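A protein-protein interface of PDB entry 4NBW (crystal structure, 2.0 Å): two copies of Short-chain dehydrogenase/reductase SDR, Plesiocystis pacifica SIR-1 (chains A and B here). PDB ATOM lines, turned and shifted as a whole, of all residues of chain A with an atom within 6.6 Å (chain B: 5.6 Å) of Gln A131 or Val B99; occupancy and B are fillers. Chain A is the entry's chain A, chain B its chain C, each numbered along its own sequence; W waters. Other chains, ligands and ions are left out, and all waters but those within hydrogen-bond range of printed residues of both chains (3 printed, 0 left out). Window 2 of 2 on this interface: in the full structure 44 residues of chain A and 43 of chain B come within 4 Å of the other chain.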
ATOM      1  N   GLU A  70      -5.358 -16.334   9.298  1.00  0.00           N
ATOM      2  CA  GLU A  70      -4.048 -15.919   8.777  1.00  0.00           C
ATOM      3  C   GLU A  70      -3.637 -14.518   9.246  1.00  0.00           C
ATOM      4  O   GLU A  70      -2.513 -14.341   9.719  1.00  0.00           O
ATOM      5  CB  GLU A  70      -4.025 -15.966   7.249  1.00  0.00           C
ATOM      6  CG  GLU A  70      -3.666 -17.350   6.688  1.00  0.00           C
ATOM      7  CD  GLU A  70      -2.166 -17.695   6.820  1.00  0.00           C
ATOM      8  OE1 GLU A  70      -1.617 -17.681   7.960  1.00  0.00           O
ATOM      9  OE2 GLU A  70      -1.530 -17.978   5.770  1.00  0.00           O
ATOM     10  N   LEU A  86      -0.381 -23.476  20.738  1.00  0.00           N
ATOM     11  CA  LEU A  86      -1.732 -23.312  20.219  1.00  0.00           C
ATOM     12  C   LEU A  86      -2.651 -24.307  20.887  1.00  0.00           C
ATOM     13  O   LEU A  86      -2.401 -25.514  20.798  1.00  0.00           O
ATOM     14  CB  LEU A  86      -1.783 -23.553  18.714  1.00  0.00           C
ATOM     15  CG  LEU A  86      -3.173 -23.520  18.084  1.00  0.00           C
ATOM     16  CD1 LEU A  86      -3.929 -22.206  18.355  1.00  0.00           C
ATOM     17  CD2 LEU A  86      -3.071 -23.768  16.592  1.00  0.00           C
ATOM     18  N   VAL A 126      -9.758 -26.414  13.381  1.00  0.00           N
ATOM     19  CA  VAL A 126      -8.556 -26.936  14.011  1.00  0.00           C
ATOM     20  C   VAL A 126      -7.445 -27.041  12.956  1.00  0.00           C
ATOM     21  O   VAL A 126      -6.274 -26.749  13.237  1.00  0.00           O
ATOM     22  CB  VAL A 126      -8.811 -28.304  14.697  1.00  0.00           C
ATOM     23  CG1 VAL A 126      -7.595 -28.783  15.402  1.00  0.00           C
ATOM     24  CG2 VAL A 126      -9.890 -28.175  15.703  1.00  0.00           C
ATOM     25  N   PHE A 127      -7.845 -27.439  11.741  1.00  0.00           N
ATOM     26  CA  PHE A 127      -6.944 -27.546  10.588  1.00  0.00           C
ATOM     27  C   PHE A 127      -6.369 -26.157  10.231  1.00  0.00           C
ATOM     28  O   PHE A 127      -5.159 -25.996  10.082  1.00  0.00           O
ATOM     29  CB  PHE A 127      -7.697 -28.176   9.399  1.00  0.00           C
ATOM     30  CG  PHE A 127      -7.139 -27.818   8.044  1.00  0.00           C
ATOM     31  CD1 PHE A 127      -6.042 -28.503   7.510  1.00  0.00           C
ATOM     32  CD2 PHE A 127      -7.726 -26.815   7.288  1.00  0.00           C
ATOM     33  CE1 PHE A 127      -5.522 -28.157   6.243  1.00  0.00           C
ATOM     34  CE2 PHE A 127      -7.223 -26.475   6.034  1.00  0.00           C
ATOM     35  CZ  PHE A 127      -6.112 -27.142   5.510  1.00  0.00           C
ATOM     36  N   LEU A 128      -7.240 -25.164  10.090  1.00  0.00           N
ATOM     37  CA  LEU A 128      -6.814 -23.835   9.654  1.00  0.00           C
ATOM     38  C   LEU A 128      -5.837 -23.204  10.660  1.00  0.00           C
ATOM     39  O   LEU A 128      -4.773 -22.727  10.276  1.00  0.00           O
ATOM     40  CB  LEU A 128      -8.039 -22.917   9.440  1.00  0.00           C
ATOM     41  CG  LEU A 128      -8.926 -23.238   8.228  1.00  0.00           C
ATOM     42  CD1 LEU A 128     -10.207 -22.445   8.281  1.00  0.00           C
ATOM     43  CD2 LEU A 128      -8.219 -22.975   6.904  1.00  0.00           C
ATOM     44  N   CYS A 129      -6.209 -23.215  11.944  1.00  0.00           N
ATOM     45  CA  CYS A 129      -5.385 -22.634  13.004  1.00  0.00           C
ATOM     46  C   CYS A 129      -4.015 -23.286  13.095  1.00  0.00           C
ATOM     47  O   CYS A 129      -2.986 -22.618  13.115  1.00  0.00           O
ATOM     48  CB  CYS A 129      -6.093 -22.753  14.337  1.00  0.00           C
ATOM     49  SG  CYS A 129      -7.500 -21.637  14.466  1.00  0.00           S
ATOM     50  N   THR A 130      -3.989 -24.602  13.180  1.00  0.00           N
ATOM     51  CA  THR A 130      -2.725 -25.300  13.244  1.00  0.00           C
ATOM     52  C   THR A 130      -1.891 -24.964  11.998  1.00  0.00           C
ATOM     53  O   THR A 130      -0.702 -24.636  12.086  1.00  0.00           O
ATOM     54  CB  THR A 130      -2.967 -26.792  13.376  1.00  0.00           C
ATOM     55  OG1 THR A 130      -3.786 -27.017  14.527  1.00  0.00           O
ATOM     56  CG2 THR A 130      -1.665 -27.542  13.538  1.00  0.00           C
ATOM     57  N   GLN A 131      -2.522 -24.997  10.838  1.00  0.00           N
ATOM     58  CA  GLN A 131      -1.788 -24.770   9.605  1.00  0.00           C
ATOM     59  C   GLN A 131      -1.130 -23.390   9.606  1.00  0.00           C
ATOM     60  O   GLN A 131      -0.025 -23.229   9.068  1.00  0.00           O
ATOM     61  CB  GLN A 131      -2.694 -24.921   8.392  1.00  0.00           C
ATOM     62  CG  GLN A 131      -1.945 -24.791   7.086  1.00  0.00           C
ATOM     63  CD  GLN A 131      -2.837 -24.995   5.897  1.00  0.00           C
ATOM     64  OE1 GLN A 131      -3.756 -24.222   5.677  1.00  0.00           O
ATOM     65  NE2 GLN A 131      -2.573 -26.056   5.126  1.00  0.00           N
ATOM     66  N   ALA A 132      -1.778 -22.409  10.243  1.00  0.00           N
ATOM     67  CA  ALA A 132      -1.264 -21.046  10.212  1.00  0.00           C
ATOM     68  C   ALA A 132      -0.106 -20.818  11.187  1.00  0.00           C
ATOM     69  O   ALA A 132       0.807 -20.044  10.870  1.00  0.00           O
ATOM     70  CB  ALA A 132      -2.375 -20.052  10.475  1.00  0.00           C
ATOM     71  N   VAL A 133      -0.096 -21.465  12.356  1.00  0.00           N
ATOM     72  CA  VAL A 133       0.978 -21.178  13.288  1.00  0.00           C
ATOM     73  C   VAL A 133       2.137 -22.122  13.022  1.00  0.00           C
ATOM     74  O   VAL A 133       3.267 -21.835  13.409  1.00  0.00           O
ATOM     75  CB  VAL A 133       0.538 -21.246  14.802  1.00  0.00           C
ATOM     76  CG1 VAL A 133      -0.915 -20.920  14.961  1.00  0.00           C
ATOM     77  CG2 VAL A 133       0.859 -22.558  15.447  1.00  0.00           C
ATOM     78  N   ALA A 134       1.858 -23.232  12.335  1.00  0.00           N
ATOM     79  CA  ALA A 134       2.833 -24.291  12.140  1.00  0.00           C
ATOM     80  C   ALA A 134       4.169 -23.799  11.590  1.00  0.00           C
ATOM     81  O   ALA A 134       5.217 -24.173  12.124  1.00  0.00           O
ATOM     82  CB  ALA A 134       2.254 -25.378  11.217  1.00  0.00           C
ATOM     83  N   PRO A 135       4.146 -22.957  10.537  1.00  0.00           N
ATOM     84  CA  PRO A 135       5.418 -22.508   9.955  1.00  0.00           C
ATOM     85  C   PRO A 135       6.251 -21.690  10.939  1.00  0.00           C
ATOM     86  O   PRO A 135       7.475 -21.677  10.868  1.00  0.00           O
ATOM     87  CB  PRO A 135       4.979 -21.636   8.768  1.00  0.00           C
ATOM     88  CG  PRO A 135       3.549 -22.022   8.501  1.00  0.00           C
ATOM     89  CD  PRO A 135       2.989 -22.382   9.827  1.00  0.00           C
ATOM     90  N   ILE A 138       7.905 -24.221  13.237  1.00  0.00           N
ATOM     91  CA  ILE A 138       9.009 -24.859  12.517  1.00  0.00           C
ATOM     92  C   ILE A 138      10.324 -24.010  12.504  1.00  0.00           C
ATOM     93  O   ILE A 138      11.385 -24.518  12.893  1.00  0.00           O
ATOM     94  CB  ILE A 138       8.564 -25.205  11.083  1.00  0.00           C
ATOM     95  CG1 ILE A 138       7.603 -26.390  11.112  1.00  0.00           C
ATOM     96  CG2 ILE A 138       9.755 -25.573  10.176  1.00  0.00           C
ATOM     97  CD1 ILE A 138       6.864 -26.663   9.751  1.00  0.00           C
ATOM     98  N   TRP A 177      -0.244 -34.850  12.363  1.00  0.00           N
ATOM     99  CA  TRP A 177       0.603 -33.714  12.637  1.00  0.00           C
ATOM    100  C   TRP A 177       1.762 -34.081  13.530  1.00  0.00           C
ATOM    101  O   TRP A 177       2.874 -33.582  13.334  1.00  0.00           O
ATOM    102  CB  TRP A 177      -0.229 -32.595  13.240  1.00  0.00           C
ATOM    103  CG  TRP A 177      -1.265 -32.161  12.289  1.00  0.00           C
ATOM    104  CD1 TRP A 177      -1.294 -32.410  10.936  1.00  0.00           C
ATOM    105  CD2 TRP A 177      -2.443 -31.440  12.590  1.00  0.00           C
ATOM    106  NE1 TRP A 177      -2.425 -31.873  10.383  1.00  0.00           N
ATOM    107  CE2 TRP A 177      -3.144 -31.259  11.375  1.00  0.00           C
ATOM    108  CE3 TRP A 177      -2.975 -30.897  13.758  1.00  0.00           C
ATOM    109  CZ2 TRP A 177      -4.351 -30.567  11.306  1.00  0.00           C
ATOM    110  CZ3 TRP A 177      -4.174 -30.212  13.682  1.00  0.00           C
ATOM    111  CH2 TRP A 177      -4.849 -30.060  12.466  1.00  0.00           C
ATOM    112  N   GLU A 180       4.223 -35.329  11.199  1.00  0.00           N
ATOM    113  CA  GLU A 180       4.792 -34.361  10.286  1.00  0.00           C
ATOM    114  C   GLU A 180       5.726 -33.348  10.992  1.00  0.00           C
ATOM    115  O   GLU A 180       6.687 -32.849  10.393  1.00  0.00           O
ATOM    116  CB  GLU A 180       3.671 -33.630   9.553  1.00  0.00           C
ATOM    117  CG  GLU A 180       2.927 -34.512   8.626  1.00  0.00           C
ATOM    118  CD  GLU A 180       1.894 -33.790   7.808  1.00  0.00           C
ATOM    119  OE1 GLU A 180       1.773 -32.569   7.967  1.00  0.00           O
ATOM    120  OE2 GLU A 180       1.205 -34.475   7.004  1.00  0.00           O
ATOM    121  N   LEU A 181       5.447 -33.064  12.261  1.00  0.00           N
ATOM    122  CA  LEU A 181       6.061 -31.908  12.932  1.00  0.00           C
ATOM    123  C   LEU A 181       7.086 -32.263  14.010  1.00  0.00           C
ATOM    124  O   LEU A 181       7.840 -31.399  14.470  1.00  0.00           O
ATOM    125  CB  LEU A 181       4.950 -31.028  13.529  1.00  0.00           C
ATOM    126  CG  LEU A 181       3.965 -30.458  12.506  1.00  0.00           C
ATOM    127  CD1 LEU A 181       2.885 -29.542  13.169  1.00  0.00           C
ATOM    128  CD2 LEU A 181       4.687 -29.725  11.372  1.00  0.00           C
ATOM    129  N   TYR A 184      10.720 -31.163  13.808  1.00  0.00           N
ATOM    130  CA  TYR A 184      10.997 -29.750  14.067  1.00  0.00           C
ATOM    131  C   TYR A 184      10.809 -29.299  15.512  1.00  0.00           C
ATOM    132  O   TYR A 184      10.751 -28.096  15.782  1.00  0.00           O
ATOM    133  CB  TYR A 184      10.100 -28.897  13.179  1.00  0.00           C
ATOM    134  CG  TYR A 184      10.201 -29.223  11.718  1.00  0.00           C
ATOM    135  CD1 TYR A 184      11.419 -29.157  11.055  1.00  0.00           C
ATOM    136  CD2 TYR A 184       9.076 -29.567  10.983  1.00  0.00           C
ATOM    137  CE1 TYR A 184      11.520 -29.452   9.701  1.00  0.00           C
ATOM    138  CE2 TYR A 184       9.178 -29.856   9.616  1.00  0.00           C
ATOM    139  CZ  TYR A 184      10.406 -29.787   9.002  1.00  0.00           C
ATOM    140  OH  TYR A 184      10.499 -30.065   7.685  1.00  0.00           O
ATOM    141  N   GLN B  97       1.561 -32.680   2.874  1.00  0.00           N
ATOM    142  CA  GLN B  97       1.911 -32.098   4.169  1.00  0.00           C
ATOM    143  C   GLN B  97       0.991 -30.906   4.516  1.00  0.00           C
ATOM    144  O   GLN B  97       0.548 -30.162   3.630  1.00  0.00           O
ATOM    145  CB  GLN B  97       3.371 -31.637   4.167  1.00  0.00           C
ATOM    146  CG  GLN B  97       4.429 -32.757   4.188  1.00  0.00           C
ATOM    147  CD  GLN B  97       5.857 -32.227   4.153  1.00  0.00           C
ATOM    148  OE1 GLN B  97       6.089 -31.045   4.362  1.00  0.00           O
ATOM    149  NE2 GLN B  97       6.817 -33.109   3.957  1.00  0.00           N
ATOM    150  N   LEU B  98       0.690 -30.738   5.801  1.00  0.00           N
ATOM    151  CA  LEU B  98      -0.061 -29.563   6.282  1.00  0.00           C
ATOM    152  C   LEU B  98       0.589 -28.285   5.791  1.00  0.00           C
ATOM    153  O   LEU B  98      -0.070 -27.398   5.258  1.00  0.00           O
ATOM    154  CB  LEU B  98      -0.121 -29.551   7.812  1.00  0.00           C
ATOM    155  CG  LEU B  98      -0.930 -28.447   8.490  1.00  0.00           C
ATOM    156  CD1 LEU B  98      -2.427 -28.686   8.356  1.00  0.00           C
ATOM    157  CD2 LEU B  98      -0.555 -28.333   9.958  1.00  0.00           C
ATOM    158  N   VAL B  99       1.893 -28.180   6.022  1.00  0.00           N
ATOM    159  CA  VAL B  99       2.695 -27.100   5.440  1.00  0.00           C
ATOM    160  C   VAL B  99       4.065 -27.631   5.052  1.00  0.00           C
ATOM    161  O   VAL B  99       4.565 -28.606   5.626  1.00  0.00           O
ATOM    162  CB  VAL B  99       2.874 -25.900   6.400  1.00  0.00           C
ATOM    163  CG1 VAL B  99       1.532 -25.175   6.625  1.00  0.00           C
ATOM    164  CG2 VAL B  99       3.487 -26.337   7.723  1.00  0.00           C
ATOM    165  N   LYS B 100       4.662 -26.986   4.063  1.00  0.00           N
ATOM    166  CA  LYS B 100       5.980 -27.359   3.588  1.00  0.00           C
ATOM    167  C   LYS B 100       6.870 -26.122   3.580  1.00  0.00           C
ATOM    168  O   LYS B 100       6.698 -25.234   2.760  1.00  0.00           O
ATOM    169  CB  LYS B 100       5.882 -27.981   2.199  1.00  0.00           C
ATOM    170  CG  LYS B 100       6.926 -29.050   1.931  1.00  0.00           C
ATOM    171  CD  LYS B 100       8.075 -28.491   1.142  1.00  0.00           C
ATOM    172  CE  LYS B 100       7.829 -28.628  -0.363  1.00  0.00           C
ATOM    173  NZ  LYS B 100       7.871 -30.047  -0.823  1.00  0.00           N
ATOM    174  N   VAL B 101       7.826 -26.080   4.503  1.00  0.00           N
ATOM    175  CA  VAL B 101       8.671 -24.892   4.718  1.00  0.00           C
ATOM    176  C   VAL B 101      10.107 -25.040   4.168  1.00  0.00           C
ATOM    177  O   VAL B 101      10.808 -26.011   4.464  1.00  0.00           O
ATOM    178  CB  VAL B 101       8.738 -24.563   6.232  1.00  0.00           C
ATOM    179  CG1 VAL B 101       9.740 -23.501   6.519  1.00  0.00           C
ATOM    180  CG2 VAL B 101       7.384 -24.125   6.733  1.00  0.00           C
ATOM    181  N   VAL B 106       6.808 -20.738   3.378  1.00  0.00           N
ATOM    182  CA  VAL B 106       5.946 -21.832   2.969  1.00  0.00           C
ATOM    183  C   VAL B 106       5.959 -21.972   1.445  1.00  0.00           C
ATOM    184  O   VAL B 106       5.503 -21.093   0.728  1.00  0.00           O
ATOM    185  CB  VAL B 106       4.512 -21.621   3.491  1.00  0.00           C
ATOM    186  CG1 VAL B 106       3.591 -22.698   2.982  1.00  0.00           C
ATOM    187  CG2 VAL B 106       4.518 -21.628   5.013  1.00  0.00           C
ATOM    188  N   LYS B 108       4.798 -24.979  -0.017  1.00  0.00           N
ATOM    189  CA  LYS B 108       3.570 -25.718  -0.301  1.00  0.00           C
ATOM    190  C   LYS B 108       2.761 -25.962   0.970  1.00  0.00           C
ATOM    191  O   LYS B 108       3.316 -26.028   2.067  1.00  0.00           O
ATOM    192  CB  LYS B 108       3.873 -27.056  -0.972  1.00  0.00           C
ATOM    193  CG  LYS B 108       2.791 -27.487  -1.938  1.00  0.00           C
ATOM    194  CD  LYS B 108       3.009 -28.877  -2.571  1.00  0.00           C
ATOM    195  CE  LYS B 108       4.293 -28.990  -3.355  1.00  0.00           C
ATOM    196  NZ  LYS B 108       4.294 -28.268  -4.672  1.00  0.00           N
ATOM    197  N   LYS B 109       1.448 -26.078   0.804  1.00  0.00           N
ATOM    198  CA  LYS B 109       0.562 -26.365   1.914  1.00  0.00           C
ATOM    199  C   LYS B 109      -0.714 -26.997   1.396  1.00  0.00           C
ATOM    200  O   LYS B 109      -1.144 -26.717   0.277  1.00  0.00           O
ATOM    201  CB  LYS B 109       0.242 -25.092   2.727  1.00  0.00           C
ATOM    202  CG  LYS B 109      -0.700 -24.092   2.061  1.00  0.00           C
ATOM    203  CD  LYS B 109      -1.227 -23.086   3.072  1.00  0.00           C
ATOM    204  CE  LYS B 109      -2.245 -22.141   2.480  1.00  0.00           C
ATOM    205  NZ  LYS B 109      -2.572 -21.073   3.481  1.00  0.00           N
ATOM    206  N   MET B 110      -1.311 -27.855   2.220  1.00  0.00           N
ATOM    207  CA  MET B 110      -2.602 -28.442   1.906  1.00  0.00           C
ATOM    208  C   MET B 110      -3.645 -27.358   1.705  1.00  0.00           C
ATOM    209  O   MET B 110      -4.042 -26.680   2.653  1.00  0.00           O
ATOM    210  CB  MET B 110      -3.053 -29.380   3.017  1.00  0.00           C
ATOM    211  CG  MET B 110      -4.476 -29.950   2.800  1.00  0.00           C
ATOM    212  SD  MET B 110      -4.851 -31.358   3.855  1.00  0.00           S
ATOM    213  CE  MET B 110      -3.871 -32.642   3.091  1.00  0.00           C
ATOM    214  N   ALA B 111      -4.105 -27.204   0.475  1.00  0.00           N
ATOM    215  CA  ALA B 111      -5.032 -26.144   0.156  1.00  0.00           C
ATOM    216  C   ALA B 111      -6.360 -26.397   0.861  1.00  0.00           C
ATOM    217  O   ALA B 111      -6.761 -27.554   1.072  1.00  0.00           O
ATOM    218  CB  ALA B 111      -5.233 -26.040  -1.360  1.00  0.00           C
HETATM  219  O   HOH W   1      -5.664 -24.343   3.597  1.00  0.00           O
HETATM  220  O   HOH W   2       3.346 -30.153   8.146  1.00  0.00           O
HETATM  221  O   HOH W   3       8.618 -28.455   6.673  1.00  0.00           O
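The side-chain amino group (NZ) of Lys B109 lies within salt-bridge range of the side-chain carboxylate (OE2) of Glu A70 (3.99 Å). The side-chain amide nitrogen (NE2) of Gln A131 is in hydrogen-bond range of the backbone carbonyl oxygen (O) of Leu B98 (2.8 Å). The side-chain amide nitrogen (NE2) of Gln A131 lies within hydrogen-bond range of the backbone carbonyl oxygen (O) of Met B110 (2.9 Å). The side-chain carboxylate of Glu A180 is in hydrogen-bond range of the backbone NH of Leu B98 (3.0 Å).
Of chain A, only Gln A131, Ala A134 and Ile A138 come within 4 Å of Val B99. Printed residues of chain A within 4 Å of Gln B97: Glu A180 (3.8 Å). Of the printed residues of chain A, Lys B109 touches Glu A70 and Gln A131. Of the printed residues of chain A, Val B101 touches Ile A138 (3.98 Å). The nearest residue of chain B that does not touch Gln A131 is Ala B111 (5.0 Å). The nearest residue of chain A that does not touch Val B99 is Pro A135 (4.2 Å). The nearest printed residue of chain A that does not touch Gln B97 is Gln A131 (5.4 Å).
Water W3 lies within hydrogen-bond range of OH of Tyr A184 (2.7 Å) and N of Val B101 (3.3 Å). Water W1 bridges the side-chain amide oxygen of Gln A131 and the backbone carbonyl oxygen of Met B110. Water W2 bridges the side-chain carboxylate (OE1) of Glu A180 (2.9 Å) and the backbone carbonyl oxygen (O) of Val B99 (3.2 Å).
Hydrophobic or aromatic side chains of chain A within 4 Å of the printed part of chain B: Phe A127, Ala A134, Pro A135, Ile A138 and Trp A177. Of the 10 printed residues of chain B, 7 touch a printed residue of chain A. Hydrophobic or aromatic side chains of chain B within 4 Å of the printed part of chain A: Leu B98, Val B99, Val B101, Val B106 and Met B110. Among the printed residues, 15 pairs touch across the chains. Among the printed residues, Asp or Glu carboxylates within 4 Å of a Lys or Arg side-chain nitrogen of the other chain: Glu A70 with Lys B109 (3.99 Å).
Among the printed residues, merely in contact across the chains: Gln A131 with Val B99 (3.5 Å), Phe A127 with Met B110 (3.6 Å), Pro A135 with Val B106 (3.6 Å), Phe A127 with Leu B98 (3.7 Å), Glu A180 with Gln B97 (3.8 Å), Gln A131 with Lys B109 (3.8 Å), Trp A177 with Leu B98 (3.8 Å), Ala A134 with Val B99 (3.8 Å), Thr A130 with Leu B98 (3.8 Å), Ile A138 with Val B99 (3.95 Å) and Ile A138 with Val B101 (3.98 Å).
The backbone carbonyl oxygen of Val A126 sits at hydrogen-bond distance from the side-chain hydroxyl of Thr A130 (2.8 Å). The side-chain amide oxygen (OE1) of Gln B97 lies close to the backbone carbonyl oxygen (O) of Val B99 (3.1 Å). The backbone carbonyl oxygen of Gln B97 lies within hydrogen-bond range of the backbone NH of Met B110 (3.3 Å). The backbone NH (N) of Met B110 sits at hydrogen-bond distance from the backbone carbonyl oxygen (O) of Leu B98 (3.3 Å).
No position is printed for both chains.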
